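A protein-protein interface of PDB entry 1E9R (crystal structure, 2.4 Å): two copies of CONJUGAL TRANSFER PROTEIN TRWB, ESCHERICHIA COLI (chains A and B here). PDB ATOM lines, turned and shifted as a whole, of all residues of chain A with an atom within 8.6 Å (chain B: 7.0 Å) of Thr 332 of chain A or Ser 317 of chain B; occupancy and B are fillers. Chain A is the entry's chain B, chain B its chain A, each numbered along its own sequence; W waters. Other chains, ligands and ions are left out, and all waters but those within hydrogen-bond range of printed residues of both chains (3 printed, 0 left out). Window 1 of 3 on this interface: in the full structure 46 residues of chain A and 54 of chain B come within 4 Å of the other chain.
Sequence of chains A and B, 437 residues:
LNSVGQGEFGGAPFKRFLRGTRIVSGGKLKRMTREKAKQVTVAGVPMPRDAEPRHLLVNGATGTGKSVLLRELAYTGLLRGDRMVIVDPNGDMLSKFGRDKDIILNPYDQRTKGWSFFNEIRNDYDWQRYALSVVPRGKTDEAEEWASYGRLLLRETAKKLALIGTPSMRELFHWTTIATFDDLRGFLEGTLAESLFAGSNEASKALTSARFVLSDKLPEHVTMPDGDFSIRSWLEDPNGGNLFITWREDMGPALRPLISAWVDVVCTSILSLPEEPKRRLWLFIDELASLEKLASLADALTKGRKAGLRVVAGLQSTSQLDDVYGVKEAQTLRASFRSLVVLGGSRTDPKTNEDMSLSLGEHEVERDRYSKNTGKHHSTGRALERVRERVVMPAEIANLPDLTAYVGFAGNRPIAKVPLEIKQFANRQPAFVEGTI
The side-chain hydroxyl of Ser 319 of chain B is in hydrogen-bond range of the side-chain amide oxygen of Gln 331 of chain A, 3.2 Å away. The side-chain hydroxyl (OG1) of Thr 332 of chain A lies within hydrogen-bond range of the side-chain hydroxyl (OG) of Ser 317 of chain B (2.8 Å). NE2 of Gln 331 of chain A is in hydrogen-bond range of OD1 of Asp 349 of chain B, 2.9 Å away. The side-chain hydroxyl of Thr 352 of chain B is in hydrogen-bond range of the side-chain amide nitrogen of Gln 331 of chain A (3.4 Å). The side-chain hydroxyl of Ser 319 of chain B sits at hydrogen-bond distance from the backbone carbonyl oxygen of Lys 328 of chain A, 2.7 Å away. OE1 of Gln 316 of chain B lies within hydrogen-bond range of OG1 of Thr 302 of chain A (3.4 Å). OG1 of Thr 62 of chain B is in hydrogen-bond range of OG1 of Thr 302 of chain A, at 3.3 Å. The side-chain carboxylate (OD2) of Asp 322 of chain B is in salt-bridge range of the side-chain amino group (NZ) of Lys 328 of chain A (3.2 Å).
The side-chain hydroxyl of Thr 352 of chain B is in hydrogen-bond range of the side-chain carboxylate of Asp 349 of chain B, 2.6 Å away. OG of Ser 317 of chain B sits close to N of Ser 319 of chain B (3.3 Å). N of Gln 320 of chain B lies within hydrogen-bond range of OG of Ser 317 of chain B. The side-chain hydroxyl (OG1) of Thr 62 of chain B is in hydrogen-bond range of the side-chain amide oxygen (OE1) of Gln 316 of chain B (3.4 Å). The side-chain amide nitrogen (NE2) of Gln 320 of chain B lies within hydrogen-bond range of the backbone carbonyl oxygen (O) of Ala 289 of chain B, 3.2 Å away. N of Gln 316 of chain B sits at hydrogen-bond distance from OE1 of Glu 287 of chain B (2.9 Å).
Asp 323 of chain B touches Lys 328 of chain A. Thr 332 of chain A touches Gln 316 of chain B. OG of Ser 319 of chain B touches OG1 of Thr 332 of chain A, at 3.7 Å. OG1 of Thr 332 of chain A touches N of Gln 320 of chain B, 3.6 Å away. CB of Ala 335 of chain A touches OD2 of Asp 349 of chain B, 3.5 Å away. Gln 316 of chain B touches Ser 336 of chain A (NE2 to OG, 3.97 Å).
Thr 332 of chain A touches four residues of chain B. Of chain A, only Thr 332 comes within 4 Å of Ser 317 of chain B. Printed residues of chain B within 4 Å of Gln 331 of chain A: Ser 319 (3.2 Å), Asp 349 (2.9 Å) and Thr 352 (3.4 Å). Of the printed residues of chain A, Gln 320 of chain B touches Thr 332 (3.6 Å). Of the printed residues of chain A, Asp 322 of chain B touches Lys 328. Ala 298 of chain A touches none of the printed residues of chain B. The nearest residue of chain A that does not touch Ser 317 of chain B is Lys 328 of chain A (5.3 Å).
Of the 19 printed residues of chain A, 6 touch a printed residue of chain B. Hydrophobic or aromatic side chains of chain A that line the printed part of chain B: Ala 335.
2 positions are printed for both chains. Of the 14 pairs that touch across the chains among the printed residues, none has its exchanged pair printed and touching as well.
Water W2 bridges OD1 of Asp 349 of chain B and NH2 of Arg 334 of chain A. Water W3 bridges NE2 of Gln 331 of chain A and OG1 of Thr 352 of chain B. Water W1 lies within hydrogen-bond range of N of Glu 329 of chain A (3.1 Å), OD1 of Asp 323 of chain B (3.3 Å) and O of Tyr 325 of chain A (3.4 Å).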
ATOM      1  N   ALA A 298      -9.713  29.823 -24.206  1.00  0.00           N
ATOM      2  CA  ALA A 298      -9.705  28.371 -24.033  1.00  0.00           C
ATOM      3  C   ALA A 298      -8.701  27.651 -24.914  1.00  0.00           C
ATOM      4  O   ALA A 298      -7.946  26.807 -24.441  1.00  0.00           O
ATOM      5  CB  ALA A 298     -11.092  27.812 -24.278  1.00  0.00           C
ATOM      6  N   ASP A 299      -8.696  27.965 -26.201  1.00  0.00           N
ATOM      7  CA  ASP A 299      -7.758  27.316 -27.102  1.00  0.00           C
ATOM      8  C   ASP A 299      -6.318  27.713 -26.779  1.00  0.00           C
ATOM      9  O   ASP A 299      -5.397  26.910 -26.907  1.00  0.00           O
ATOM     10  CB  ASP A 299      -8.079  27.675 -28.550  1.00  0.00           C
ATOM     11  CG  ASP A 299      -9.452  27.212 -28.964  1.00  0.00           C
ATOM     12  OD1 ASP A 299      -9.755  26.014 -28.774  1.00  0.00           O
ATOM     13  OD2 ASP A 299     -10.223  28.051 -29.485  1.00  0.00           O
ATOM     14  N   LEU A 301      -5.109  28.358 -23.865  1.00  0.00           N
ATOM     15  CA  LEU A 301      -4.681  27.654 -22.652  1.00  0.00           C
ATOM     16  C   LEU A 301      -4.383  26.194 -22.926  1.00  0.00           C
ATOM     17  O   LEU A 301      -3.608  25.559 -22.222  1.00  0.00           O
ATOM     18  CB  LEU A 301      -5.770  27.728 -21.592  1.00  0.00           C
ATOM     19  CG  LEU A 301      -5.982  29.114 -21.000  1.00  0.00           C
ATOM     20  CD1 LEU A 301      -7.249  29.152 -20.159  1.00  0.00           C
ATOM     21  CD2 LEU A 301      -4.767  29.470 -20.170  1.00  0.00           C
ATOM     22  N   THR A 302      -4.992  25.688 -23.985  1.00  0.00           N
ATOM     23  CA  THR A 302      -4.879  24.304 -24.375  1.00  0.00           C
ATOM     24  C   THR A 302      -3.914  23.998 -25.510  1.00  0.00           C
ATOM     25  O   THR A 302      -3.285  22.943 -25.524  1.00  0.00           O
ATOM     26  CB  THR A 302      -6.275  23.813 -24.754  1.00  0.00           C
ATOM     27  OG1 THR A 302      -7.025  23.597 -23.554  1.00  0.00           O
ATOM     28  CG2 THR A 302      -6.211  22.553 -25.606  1.00  0.00           C
ATOM     29  N   LEU A 321     -17.338  34.008 -12.485  1.00  0.00           N
ATOM     30  CA  LEU A 321     -16.864  33.385 -13.720  1.00  0.00           C
ATOM     31  C   LEU A 321     -17.983  32.545 -14.347  1.00  0.00           C
ATOM     32  O   LEU A 321     -18.104  32.459 -15.578  1.00  0.00           O
ATOM     33  CB  LEU A 321     -15.664  32.492 -13.429  1.00  0.00           C
ATOM     34  CG  LEU A 321     -14.964  31.959 -14.677  1.00  0.00           C
ATOM     35  CD1 LEU A 321     -14.352  33.131 -15.450  1.00  0.00           C
ATOM     36  CD2 LEU A 321     -13.902  30.927 -14.271  1.00  0.00           C
ATOM     37  N   ASP A 322     -18.790  31.915 -13.494  1.00  0.00           N
ATOM     38  CA  ASP A 322     -19.896  31.097 -13.973  1.00  0.00           C
ATOM     39  C   ASP A 322     -20.867  32.020 -14.653  1.00  0.00           C
ATOM     40  O   ASP A 322     -21.463  31.674 -15.666  1.00  0.00           O
ATOM     41  CB  ASP A 322     -20.622  30.386 -12.824  1.00  0.00           C
ATOM     42  CG  ASP A 322     -19.826  29.222 -12.251  1.00  0.00           C
ATOM     43  OD1 ASP A 322     -18.961  28.678 -12.969  1.00  0.00           O
ATOM     44  OD2 ASP A 322     -20.078  28.838 -11.085  1.00  0.00           O
ATOM     45  N   TYR A 325     -19.074  33.058 -18.257  1.00  0.00           N
ATOM     46  CA  TYR A 325     -18.926  31.964 -19.205  1.00  0.00           C
ATOM     47  C   TYR A 325     -20.022  30.924 -19.151  1.00  0.00           C
ATOM     48  O   TYR A 325     -20.200  30.142 -20.095  1.00  0.00           O
ATOM     49  CB  TYR A 325     -17.589  31.254 -18.981  1.00  0.00           C
ATOM     50  CG  TYR A 325     -16.391  32.044 -19.418  1.00  0.00           C
ATOM     51  CD1 TYR A 325     -15.842  33.031 -18.599  1.00  0.00           C
ATOM     52  CD2 TYR A 325     -15.818  31.828 -20.674  1.00  0.00           C
ATOM     53  CE1 TYR A 325     -14.754  33.786 -19.023  1.00  0.00           C
ATOM     54  CE2 TYR A 325     -14.728  32.584 -21.109  1.00  0.00           C
ATOM     55  CZ  TYR A 325     -14.206  33.557 -20.279  1.00  0.00           C
ATOM     56  OH  TYR A 325     -13.141  34.309 -20.716  1.00  0.00           O
ATOM     57  N   GLY A 326     -20.756  30.905 -18.048  1.00  0.00           N
ATOM     58  CA  GLY A 326     -21.787  29.898 -17.893  1.00  0.00           C
ATOM     59  C   GLY A 326     -21.121  28.815 -17.080  1.00  0.00           C
ATOM     60  O   GLY A 326     -19.904  28.658 -17.148  1.00  0.00           O
ATOM     61  N   VAL A 327     -21.893  28.061 -16.315  1.00  0.00           N
ATOM     62  CA  VAL A 327     -21.307  27.033 -15.471  1.00  0.00           C
ATOM     63  C   VAL A 327     -20.423  25.980 -16.165  1.00  0.00           C
ATOM     64  O   VAL A 327     -19.315  25.713 -15.714  1.00  0.00           O
ATOM     65  CB  VAL A 327     -22.419  26.341 -14.652  1.00  0.00           C
ATOM     66  CG1 VAL A 327     -21.829  25.266 -13.770  1.00  0.00           C
ATOM     67  CG2 VAL A 327     -23.134  27.382 -13.797  1.00  0.00           C
ATOM     68  N   LYS A 328     -20.892  25.394 -17.259  1.00  0.00           N
ATOM     69  CA  LYS A 328     -20.119  24.363 -17.948  1.00  0.00           C
ATOM     70  C   LYS A 328     -18.793  24.875 -18.471  1.00  0.00           C
ATOM     71  O   LYS A 328     -17.730  24.352 -18.148  1.00  0.00           O
ATOM     72  CB  LYS A 328     -20.910  23.775 -19.128  1.00  0.00           C
ATOM     73  CG  LYS A 328     -22.201  23.057 -18.764  1.00  0.00           C
ATOM     74  CD  LYS A 328     -21.938  21.864 -17.879  1.00  0.00           C
ATOM     75  CE  LYS A 328     -23.217  21.111 -17.588  1.00  0.00           C
ATOM     76  NZ  LYS A 328     -22.956  19.997 -16.639  1.00  0.00           N
ATOM     77  N   GLU A 329     -18.866  25.910 -19.289  1.00  0.00           N
ATOM     78  CA  GLU A 329     -17.680  26.468 -19.896  1.00  0.00           C
ATOM     79  C   GLU A 329     -16.706  27.060 -18.880  1.00  0.00           C
ATOM     80  O   GLU A 329     -15.495  27.045 -19.092  1.00  0.00           O
ATOM     81  CB  GLU A 329     -18.114  27.499 -20.922  1.00  0.00           C
ATOM     82  CG  GLU A 329     -17.007  27.991 -21.806  1.00  0.00           C
ATOM     83  CD  GLU A 329     -17.526  28.602 -23.096  1.00  0.00           C
ATOM     84  OE1 GLU A 329     -18.725  28.401 -23.426  1.00  0.00           O
ATOM     85  OE2 GLU A 329     -16.721  29.272 -23.781  1.00  0.00           O
ATOM     86  N   ALA A 330     -17.233  27.569 -17.771  1.00  0.00           N
ATOM     87  CA  ALA A 330     -16.401  28.145 -16.714  1.00  0.00           C
ATOM     88  C   ALA A 330     -15.595  27.051 -16.035  1.00  0.00           C
ATOM     89  O   ALA A 330     -14.455  27.266 -15.647  1.00  0.00           O
ATOM     90  CB  ALA A 330     -17.262  28.860 -15.681  1.00  0.00           C
ATOM     91  N   GLN A 331     -16.195  25.878 -15.885  1.00  0.00           N
ATOM     92  CA  GLN A 331     -15.509  24.758 -15.266  1.00  0.00           C
ATOM     93  C   GLN A 331     -14.369  24.322 -16.171  1.00  0.00           C
ATOM     94  O   GLN A 331     -13.241  24.114 -15.718  1.00  0.00           O
ATOM     95  CB  GLN A 331     -16.469  23.600 -15.087  1.00  0.00           C
ATOM     96  CG  GLN A 331     -15.858  22.386 -14.439  1.00  0.00           C
ATOM     97  CD  GLN A 331     -16.833  21.226 -14.431  1.00  0.00           C
ATOM     98  OE1 GLN A 331     -18.027  21.410 -14.694  1.00  0.00           O
ATOM     99  NE2 GLN A 331     -16.339  20.026 -14.129  1.00  0.00           N
ATOM    100  N   THR A 332     -14.677  24.187 -17.457  1.00  0.00           N
ATOM    101  CA  THR A 332     -13.697  23.778 -18.443  1.00  0.00           C
ATOM    102  C   THR A 332     -12.542  24.763 -18.471  1.00  0.00           C
ATOM    103  O   THR A 332     -11.382  24.370 -18.640  1.00  0.00           O
ATOM    104  CB  THR A 332     -14.314  23.729 -19.829  1.00  0.00           C
ATOM    105  OG1 THR A 332     -15.424  22.826 -19.812  1.00  0.00           O
ATOM    106  CG2 THR A 332     -13.271  23.282 -20.860  1.00  0.00           C
ATOM    107  N   LEU A 333     -12.864  26.046 -18.315  1.00  0.00           N
ATOM    108  CA  LEU A 333     -11.849  27.096 -18.334  1.00  0.00           C
ATOM    109  C   LEU A 333     -10.933  26.969 -17.132  1.00  0.00           C
ATOM    110  O   LEU A 333      -9.713  26.980 -17.270  1.00  0.00           O
ATOM    111  CB  LEU A 333     -12.506  28.479 -18.340  1.00  0.00           C
ATOM    112  CG  LEU A 333     -11.560  29.664 -18.527  1.00  0.00           C
ATOM    113  CD1 LEU A 333     -10.840  29.567 -19.863  1.00  0.00           C
ATOM    114  CD2 LEU A 333     -12.359  30.937 -18.457  1.00  0.00           C
ATOM    115  N   ARG A 334     -11.530  26.844 -15.951  1.00  0.00           N
ATOM    116  CA  ARG A 334     -10.748  26.695 -14.737  1.00  0.00           C
ATOM    117  C   ARG A 334      -9.921  25.409 -14.819  1.00  0.00           C
ATOM    118  O   ARG A 334      -8.780  25.365 -14.356  1.00  0.00           O
ATOM    119  CB  ARG A 334     -11.654  26.638 -13.504  1.00  0.00           C
ATOM    120  CG  ARG A 334     -12.488  27.889 -13.258  1.00  0.00           C
ATOM    121  CD  ARG A 334     -13.050  27.910 -11.830  1.00  0.00           C
ATOM    122  NE  ARG A 334     -13.562  26.600 -11.426  1.00  0.00           N
ATOM    123  CZ  ARG A 334     -14.760  26.125 -11.748  1.00  0.00           C
ATOM    124  NH1 ARG A 334     -15.599  26.869 -12.450  1.00  0.00           N
ATOM    125  NH2 ARG A 334     -15.127  24.912 -11.346  1.00  0.00           N
ATOM    126  N   ALA A 335     -10.493  24.371 -15.420  1.00  0.00           N
ATOM    127  CA  ALA A 335      -9.800  23.100 -15.545  1.00  0.00           C
ATOM    128  C   ALA A 335      -8.646  23.185 -16.539  1.00  0.00           C
ATOM    129  O   ALA A 335      -7.858  22.245 -16.669  1.00  0.00           O
ATOM    130  CB  ALA A 335     -10.786  22.014 -15.974  1.00  0.00           C
ATOM    131  N   SER A 336      -8.546  24.309 -17.244  1.00  0.00           N
ATOM    132  CA  SER A 336      -7.486  24.482 -18.227  1.00  0.00           C
ATOM    133  C   SER A 336      -6.192  24.991 -17.596  1.00  0.00           C
ATOM    134  O   SER A 336      -5.147  25.012 -18.243  1.00  0.00           O
ATOM    135  CB  SER A 336      -7.956  25.408 -19.341  1.00  0.00           C
ATOM    136  OG  SER A 336      -9.021  24.790 -20.043  1.00  0.00           O
ATOM    137  N   PHE A 337      -6.274  25.405 -16.337  1.00  0.00           N
ATOM    138  CA  PHE A 337      -5.097  25.835 -15.600  1.00  0.00           C
ATOM    139  C   PHE A 337      -4.742  24.608 -14.744  1.00  0.00           C
ATOM    140  O   PHE A 337      -5.586  24.099 -14.001  1.00  0.00           O
ATOM    141  CB  PHE A 337      -5.416  27.004 -14.680  1.00  0.00           C
ATOM    142  CG  PHE A 337      -5.813  28.259 -15.396  1.00  0.00           C
ATOM    143  CD1 PHE A 337      -7.046  28.358 -16.024  1.00  0.00           C
ATOM    144  CD2 PHE A 337      -4.968  29.366 -15.399  1.00  0.00           C
ATOM    145  CE1 PHE A 337      -7.429  29.538 -16.634  1.00  0.00           C
ATOM    146  CE2 PHE A 337      -5.350  30.545 -16.008  1.00  0.00           C
ATOM    147  CZ  PHE A 337      -6.579  30.631 -16.623  1.00  0.00           C
ATOM    148  N   ASN B  59     -10.119  10.031 -21.256  1.00  0.00           N
ATOM    149  CA  ASN B  59     -10.482  11.207 -20.489  1.00  0.00           C
ATOM    150  C   ASN B  59      -9.312  11.774 -19.675  1.00  0.00           C
ATOM    151  O   ASN B  59      -8.706  11.078 -18.866  1.00  0.00           O
ATOM    152  CB  ASN B  59     -11.656  10.816 -19.573  1.00  0.00           C
ATOM    153  CG  ASN B  59     -12.352  12.006 -18.947  1.00  0.00           C
ATOM    154  OD1 ASN B  59     -13.074  11.851 -17.964  1.00  0.00           O
ATOM    155  ND2 ASN B  59     -12.152  13.193 -19.511  1.00  0.00           N
ATOM    156  N   GLY B  60      -9.001  13.047 -19.894  1.00  0.00           N
ATOM    157  CA  GLY B  60      -7.918  13.672 -19.159  1.00  0.00           C
ATOM    158  C   GLY B  60      -7.742  15.153 -19.449  1.00  0.00           C
ATOM    159  O   GLY B  60      -7.990  15.597 -20.568  1.00  0.00           O
ATOM    160  N   ALA B  61      -7.303  15.915 -18.447  1.00  0.00           N
ATOM    161  CA  ALA B  61      -7.083  17.352 -18.609  1.00  0.00           C
ATOM    162  C   ALA B  61      -5.977  17.632 -19.623  1.00  0.00           C
ATOM    163  O   ALA B  61      -5.326  16.713 -20.121  1.00  0.00           O
ATOM    164  CB  ALA B  61      -6.722  17.981 -17.268  1.00  0.00           C
ATOM    165  N   THR B  62      -5.763  18.908 -19.925  1.00  0.00           N
ATOM    166  CA  THR B  62      -4.733  19.288 -20.889  1.00  0.00           C
ATOM    167  C   THR B  62      -3.365  18.897 -20.360  1.00  0.00           C
ATOM    168  O   THR B  62      -3.095  19.038 -19.167  1.00  0.00           O
ATOM    169  CB  THR B  62      -4.694  20.822 -21.147  1.00  0.00           C
ATOM    170  OG1 THR B  62      -6.017  21.327 -21.309  1.00  0.00           O
ATOM    171  CG2 THR B  62      -3.921  21.122 -22.415  1.00  0.00           C
ATOM    172  N   LYS B  66      -3.000  12.637 -23.461  1.00  0.00           N
ATOM    173  CA  LYS B  66      -3.967  12.057 -24.385  1.00  0.00           C
ATOM    174  C   LYS B  66      -3.409  11.833 -25.799  1.00  0.00           C
ATOM    175  O   LYS B  66      -3.582  10.762 -26.389  1.00  0.00           O
ATOM    176  CB  LYS B  66      -5.211  12.943 -24.470  1.00  0.00           C
ATOM    177  CG  LYS B  66      -5.995  13.061 -23.177  1.00  0.00           C
ATOM    178  CD  LYS B  66      -7.331  13.775 -23.398  1.00  0.00           C
ATOM    179  CE  LYS B  66      -7.143  15.197 -23.878  1.00  0.00           C
ATOM    180  NZ  LYS B  66      -6.501  16.043 -22.832  1.00  0.00           N
ATOM    181  N   GLU B 287     -10.153  15.229 -29.877  1.00  0.00           N
ATOM    182  CA  GLU B 287     -10.997  15.825 -28.860  1.00  0.00           C
ATOM    183  C   GLU B 287     -12.435  15.804 -29.336  1.00  0.00           C
ATOM    184  O   GLU B 287     -12.815  16.506 -30.263  1.00  0.00           O
ATOM    185  CB  GLU B 287     -10.560  17.263 -28.567  1.00  0.00           C
ATOM    186  CG  GLU B 287     -11.568  18.041 -27.733  1.00  0.00           C
ATOM    187  CD  GLU B 287     -11.824  17.398 -26.388  1.00  0.00           C
ATOM    188  OE1 GLU B 287     -10.832  17.005 -25.734  1.00  0.00           O
ATOM    189  OE2 GLU B 287     -13.004  17.292 -25.984  1.00  0.00           O
ATOM    190  N   ALA B 289     -15.224  16.873 -27.805  1.00  0.00           N
ATOM    191  CA  ALA B 289     -15.986  18.096 -27.539  1.00  0.00           C
ATOM    192  C   ALA B 289     -15.618  19.326 -28.358  1.00  0.00           C
ATOM    193  O   ALA B 289     -16.230  20.375 -28.188  1.00  0.00           O
ATOM    194  CB  ALA B 289     -15.920  18.437 -26.055  1.00  0.00           C
ATOM    195  N   GLY B 314     -10.544  11.280 -27.569  1.00  0.00           N
ATOM    196  CA  GLY B 314     -10.002  11.935 -26.394  1.00  0.00           C
ATOM    197  C   GLY B 314     -11.073  12.875 -25.892  1.00  0.00           C
ATOM    198  O   GLY B 314     -11.920  13.317 -26.669  1.00  0.00           O
ATOM    199  N   LEU B 315     -11.053  13.173 -24.598  1.00  0.00           N
ATOM    200  CA  LEU B 315     -12.038  14.069 -24.003  1.00  0.00           C
ATOM    201  C   LEU B 315     -11.371  14.806 -22.857  1.00  0.00           C
ATOM    202  O   LEU B 315     -11.101  14.206 -21.829  1.00  0.00           O
ATOM    203  CB  LEU B 315     -13.233  13.266 -23.479  1.00  0.00           C
ATOM    204  CG  LEU B 315     -14.361  14.056 -22.809  1.00  0.00           C
ATOM    205  CD1 LEU B 315     -15.022  14.964 -23.835  1.00  0.00           C
ATOM    206  CD2 LEU B 315     -15.376  13.111 -22.218  1.00  0.00           C
ATOM    207  N   GLN B 316     -11.103  16.099 -23.019  1.00  0.00           N
ATOM    208  CA  GLN B 316     -10.442  16.836 -21.948  1.00  0.00           C
ATOM    209  C   GLN B 316     -11.403  17.337 -20.887  1.00  0.00           C
ATOM    210  O   GLN B 316     -11.041  17.439 -19.716  1.00  0.00           O
ATOM    211  CB  GLN B 316      -9.641  18.017 -22.495  1.00  0.00           C
ATOM    212  CG  GLN B 316     -10.457  19.243 -22.792  1.00  0.00           C
ATOM    213  CD  GLN B 316      -9.609  20.494 -22.810  1.00  0.00           C
ATOM    214  OE1 GLN B 316      -8.570  20.537 -23.479  1.00  0.00           O
ATOM    215  NE2 GLN B 316     -10.038  21.525 -22.068  1.00  0.00           N
ATOM    216  N   SER B 317     -12.625  17.654 -21.300  1.00  0.00           N
ATOM    217  CA  SER B 317     -13.625  18.148 -20.366  1.00  0.00           C
ATOM    218  C   SER B 317     -14.980  17.507 -20.596  1.00  0.00           C
ATOM    219  O   SER B 317     -15.573  17.666 -21.657  1.00  0.00           O
ATOM    220  CB  SER B 317     -13.766  19.667 -20.478  1.00  0.00           C
ATOM    221  OG  SER B 317     -14.753  20.147 -19.579  1.00  0.00           O
ATOM    222  N   THR B 318     -15.460  16.782 -19.592  1.00  0.00           N
ATOM    223  CA  THR B 318     -16.766  16.139 -19.667  1.00  0.00           C
ATOM    224  C   THR B 318     -17.827  17.261 -19.655  1.00  0.00           C
ATOM    225  O   THR B 318     -18.903  17.154 -20.252  1.00  0.00           O
ATOM    226  CB  THR B 318     -16.968  15.186 -18.463  1.00  0.00           C
ATOM    227  OG1 THR B 318     -18.209  14.491 -18.613  1.00  0.00           O
ATOM    228  CG2 THR B 318     -16.976  15.963 -17.136  1.00  0.00           C
ATOM    229  N   SER B 319     -17.484  18.346 -18.983  1.00  0.00           N
ATOM    230  CA  SER B 319     -18.338  19.505 -18.867  1.00  0.00           C
ATOM    231  C   SER B 319     -18.555  20.170 -20.231  1.00  0.00           C
ATOM    232  O   SER B 319     -19.650  20.661 -20.524  1.00  0.00           O
ATOM    233  CB  SER B 319     -17.683  20.480 -17.900  1.00  0.00           C
ATOM    234  OG  SER B 319     -18.361  21.706 -17.893  1.00  0.00           O
ATOM    235  N   GLN B 320     -17.509  20.182 -21.058  1.00  0.00           N
ATOM    236  CA  GLN B 320     -17.574  20.774 -22.390  1.00  0.00           C
ATOM    237  C   GLN B 320     -18.437  19.918 -23.313  1.00  0.00           C
ATOM    238  O   GLN B 320     -19.151  20.435 -24.162  1.00  0.00           O
ATOM    239  CB  GLN B 320     -16.177  20.900 -22.983  1.00  0.00           C
ATOM    240  CG  GLN B 320     -16.088  21.865 -24.157  1.00  0.00           C
ATOM    241  CD  GLN B 320     -14.750  21.789 -24.888  1.00  0.00           C
ATOM    242  OE1 GLN B 320     -13.748  21.305 -24.345  1.00  0.00           O
ATOM    243  NE2 GLN B 320     -14.728  22.275 -26.121  1.00  0.00           N
ATOM    244  N   LEU B 321     -18.367  18.604 -23.151  1.00  0.00           N
ATOM    245  CA  LEU B 321     -19.171  17.709 -23.962  1.00  0.00           C
ATOM    246  C   LEU B 321     -20.654  17.911 -23.611  1.00  0.00           C
ATOM    247  O   LEU B 321     -21.526  17.808 -24.476  1.00  0.00           O
ATOM    248  CB  LEU B 321     -18.763  16.255 -23.708  1.00  0.00           C
ATOM    249  CG  LEU B 321     -19.413  15.200 -24.613  1.00  0.00           C
ATOM    250  CD1 LEU B 321     -18.856  15.324 -26.030  1.00  0.00           C
ATOM    251  CD2 LEU B 321     -19.156  13.812 -24.051  1.00  0.00           C
ATOM    252  N   ASP B 322     -20.937  18.190 -22.339  1.00  0.00           N
ATOM    253  CA  ASP B 322     -22.312  18.431 -21.911  1.00  0.00           C
ATOM    254  C   ASP B 322     -22.801  19.668 -22.618  1.00  0.00           C
ATOM    255  O   ASP B 322     -23.950  19.742 -23.029  1.00  0.00           O
ATOM    256  CB  ASP B 322     -22.403  18.683 -20.406  1.00  0.00           C
ATOM    257  CG  ASP B 322     -22.283  17.413 -19.586  1.00  0.00           C
ATOM    258  OD1 ASP B 322     -22.462  16.312 -20.149  1.00  0.00           O
ATOM    259  OD2 ASP B 322     -22.020  17.518 -18.367  1.00  0.00           O
ATOM    260  N   ASP B 323     -21.914  20.646 -22.757  1.00  0.00           N
ATOM    261  CA  ASP B 323     -22.259  21.898 -23.407  1.00  0.00           C
ATOM    262  C   ASP B 323     -22.573  21.716 -24.889  1.00  0.00           C
ATOM    263  O   ASP B 323     -23.464  22.370 -25.434  1.00  0.00           O
ATOM    264  CB  ASP B 323     -21.123  22.896 -23.244  1.00  0.00           C
ATOM    265  CG  ASP B 323     -21.618  24.323 -23.187  1.00  0.00           C
ATOM    266  OD1 ASP B 323     -22.509  24.594 -22.351  1.00  0.00           O
ATOM    267  OD2 ASP B 323     -21.123  25.169 -23.970  1.00  0.00           O
ATOM    268  N   ASP B 349     -10.246  21.307 -10.832  1.00  0.00           N
ATOM    269  CA  ASP B 349     -11.511  20.731 -11.248  1.00  0.00           C
ATOM    270  C   ASP B 349     -11.869  19.510 -10.414  1.00  0.00           C
ATOM    271  O   ASP B 349     -11.926  18.391 -10.928  1.00  0.00           O
ATOM    272  CB  ASP B 349     -11.419  20.357 -12.733  1.00  0.00           C
ATOM    273  CG  ASP B 349     -12.766  20.011 -13.333  1.00  0.00           C
ATOM    274  OD1 ASP B 349     -13.801  20.197 -12.653  1.00  0.00           O
ATOM    275  OD2 ASP B 349     -12.781  19.564 -14.497  1.00  0.00           O
ATOM    276  N   THR B 352     -14.599  17.025 -11.659  1.00  0.00           N
ATOM    277  CA  THR B 352     -14.200  16.027 -12.634  1.00  0.00           C
ATOM    278  C   THR B 352     -13.414  14.898 -11.979  1.00  0.00           C
ATOM    279  O   THR B 352     -13.574  13.732 -12.350  1.00  0.00           O
ATOM    280  CB  THR B 352     -13.366  16.651 -13.757  1.00  0.00           C
ATOM    281  OG1 THR B 352     -14.223  17.438 -14.592  1.00  0.00           O
ATOM    282  CG2 THR B 352     -12.722  15.579 -14.605  1.00  0.00           C
HETATM  283  O   HOH W   1     -21.519  27.074 -20.396  1.00  0.00           O
HETATM  284  O   HOH W   2     -14.761  21.657 -10.780  1.00  0.00           O
HETATM  285  O   HOH W   3     -17.049  17.365 -14.144  1.00  0.00           O
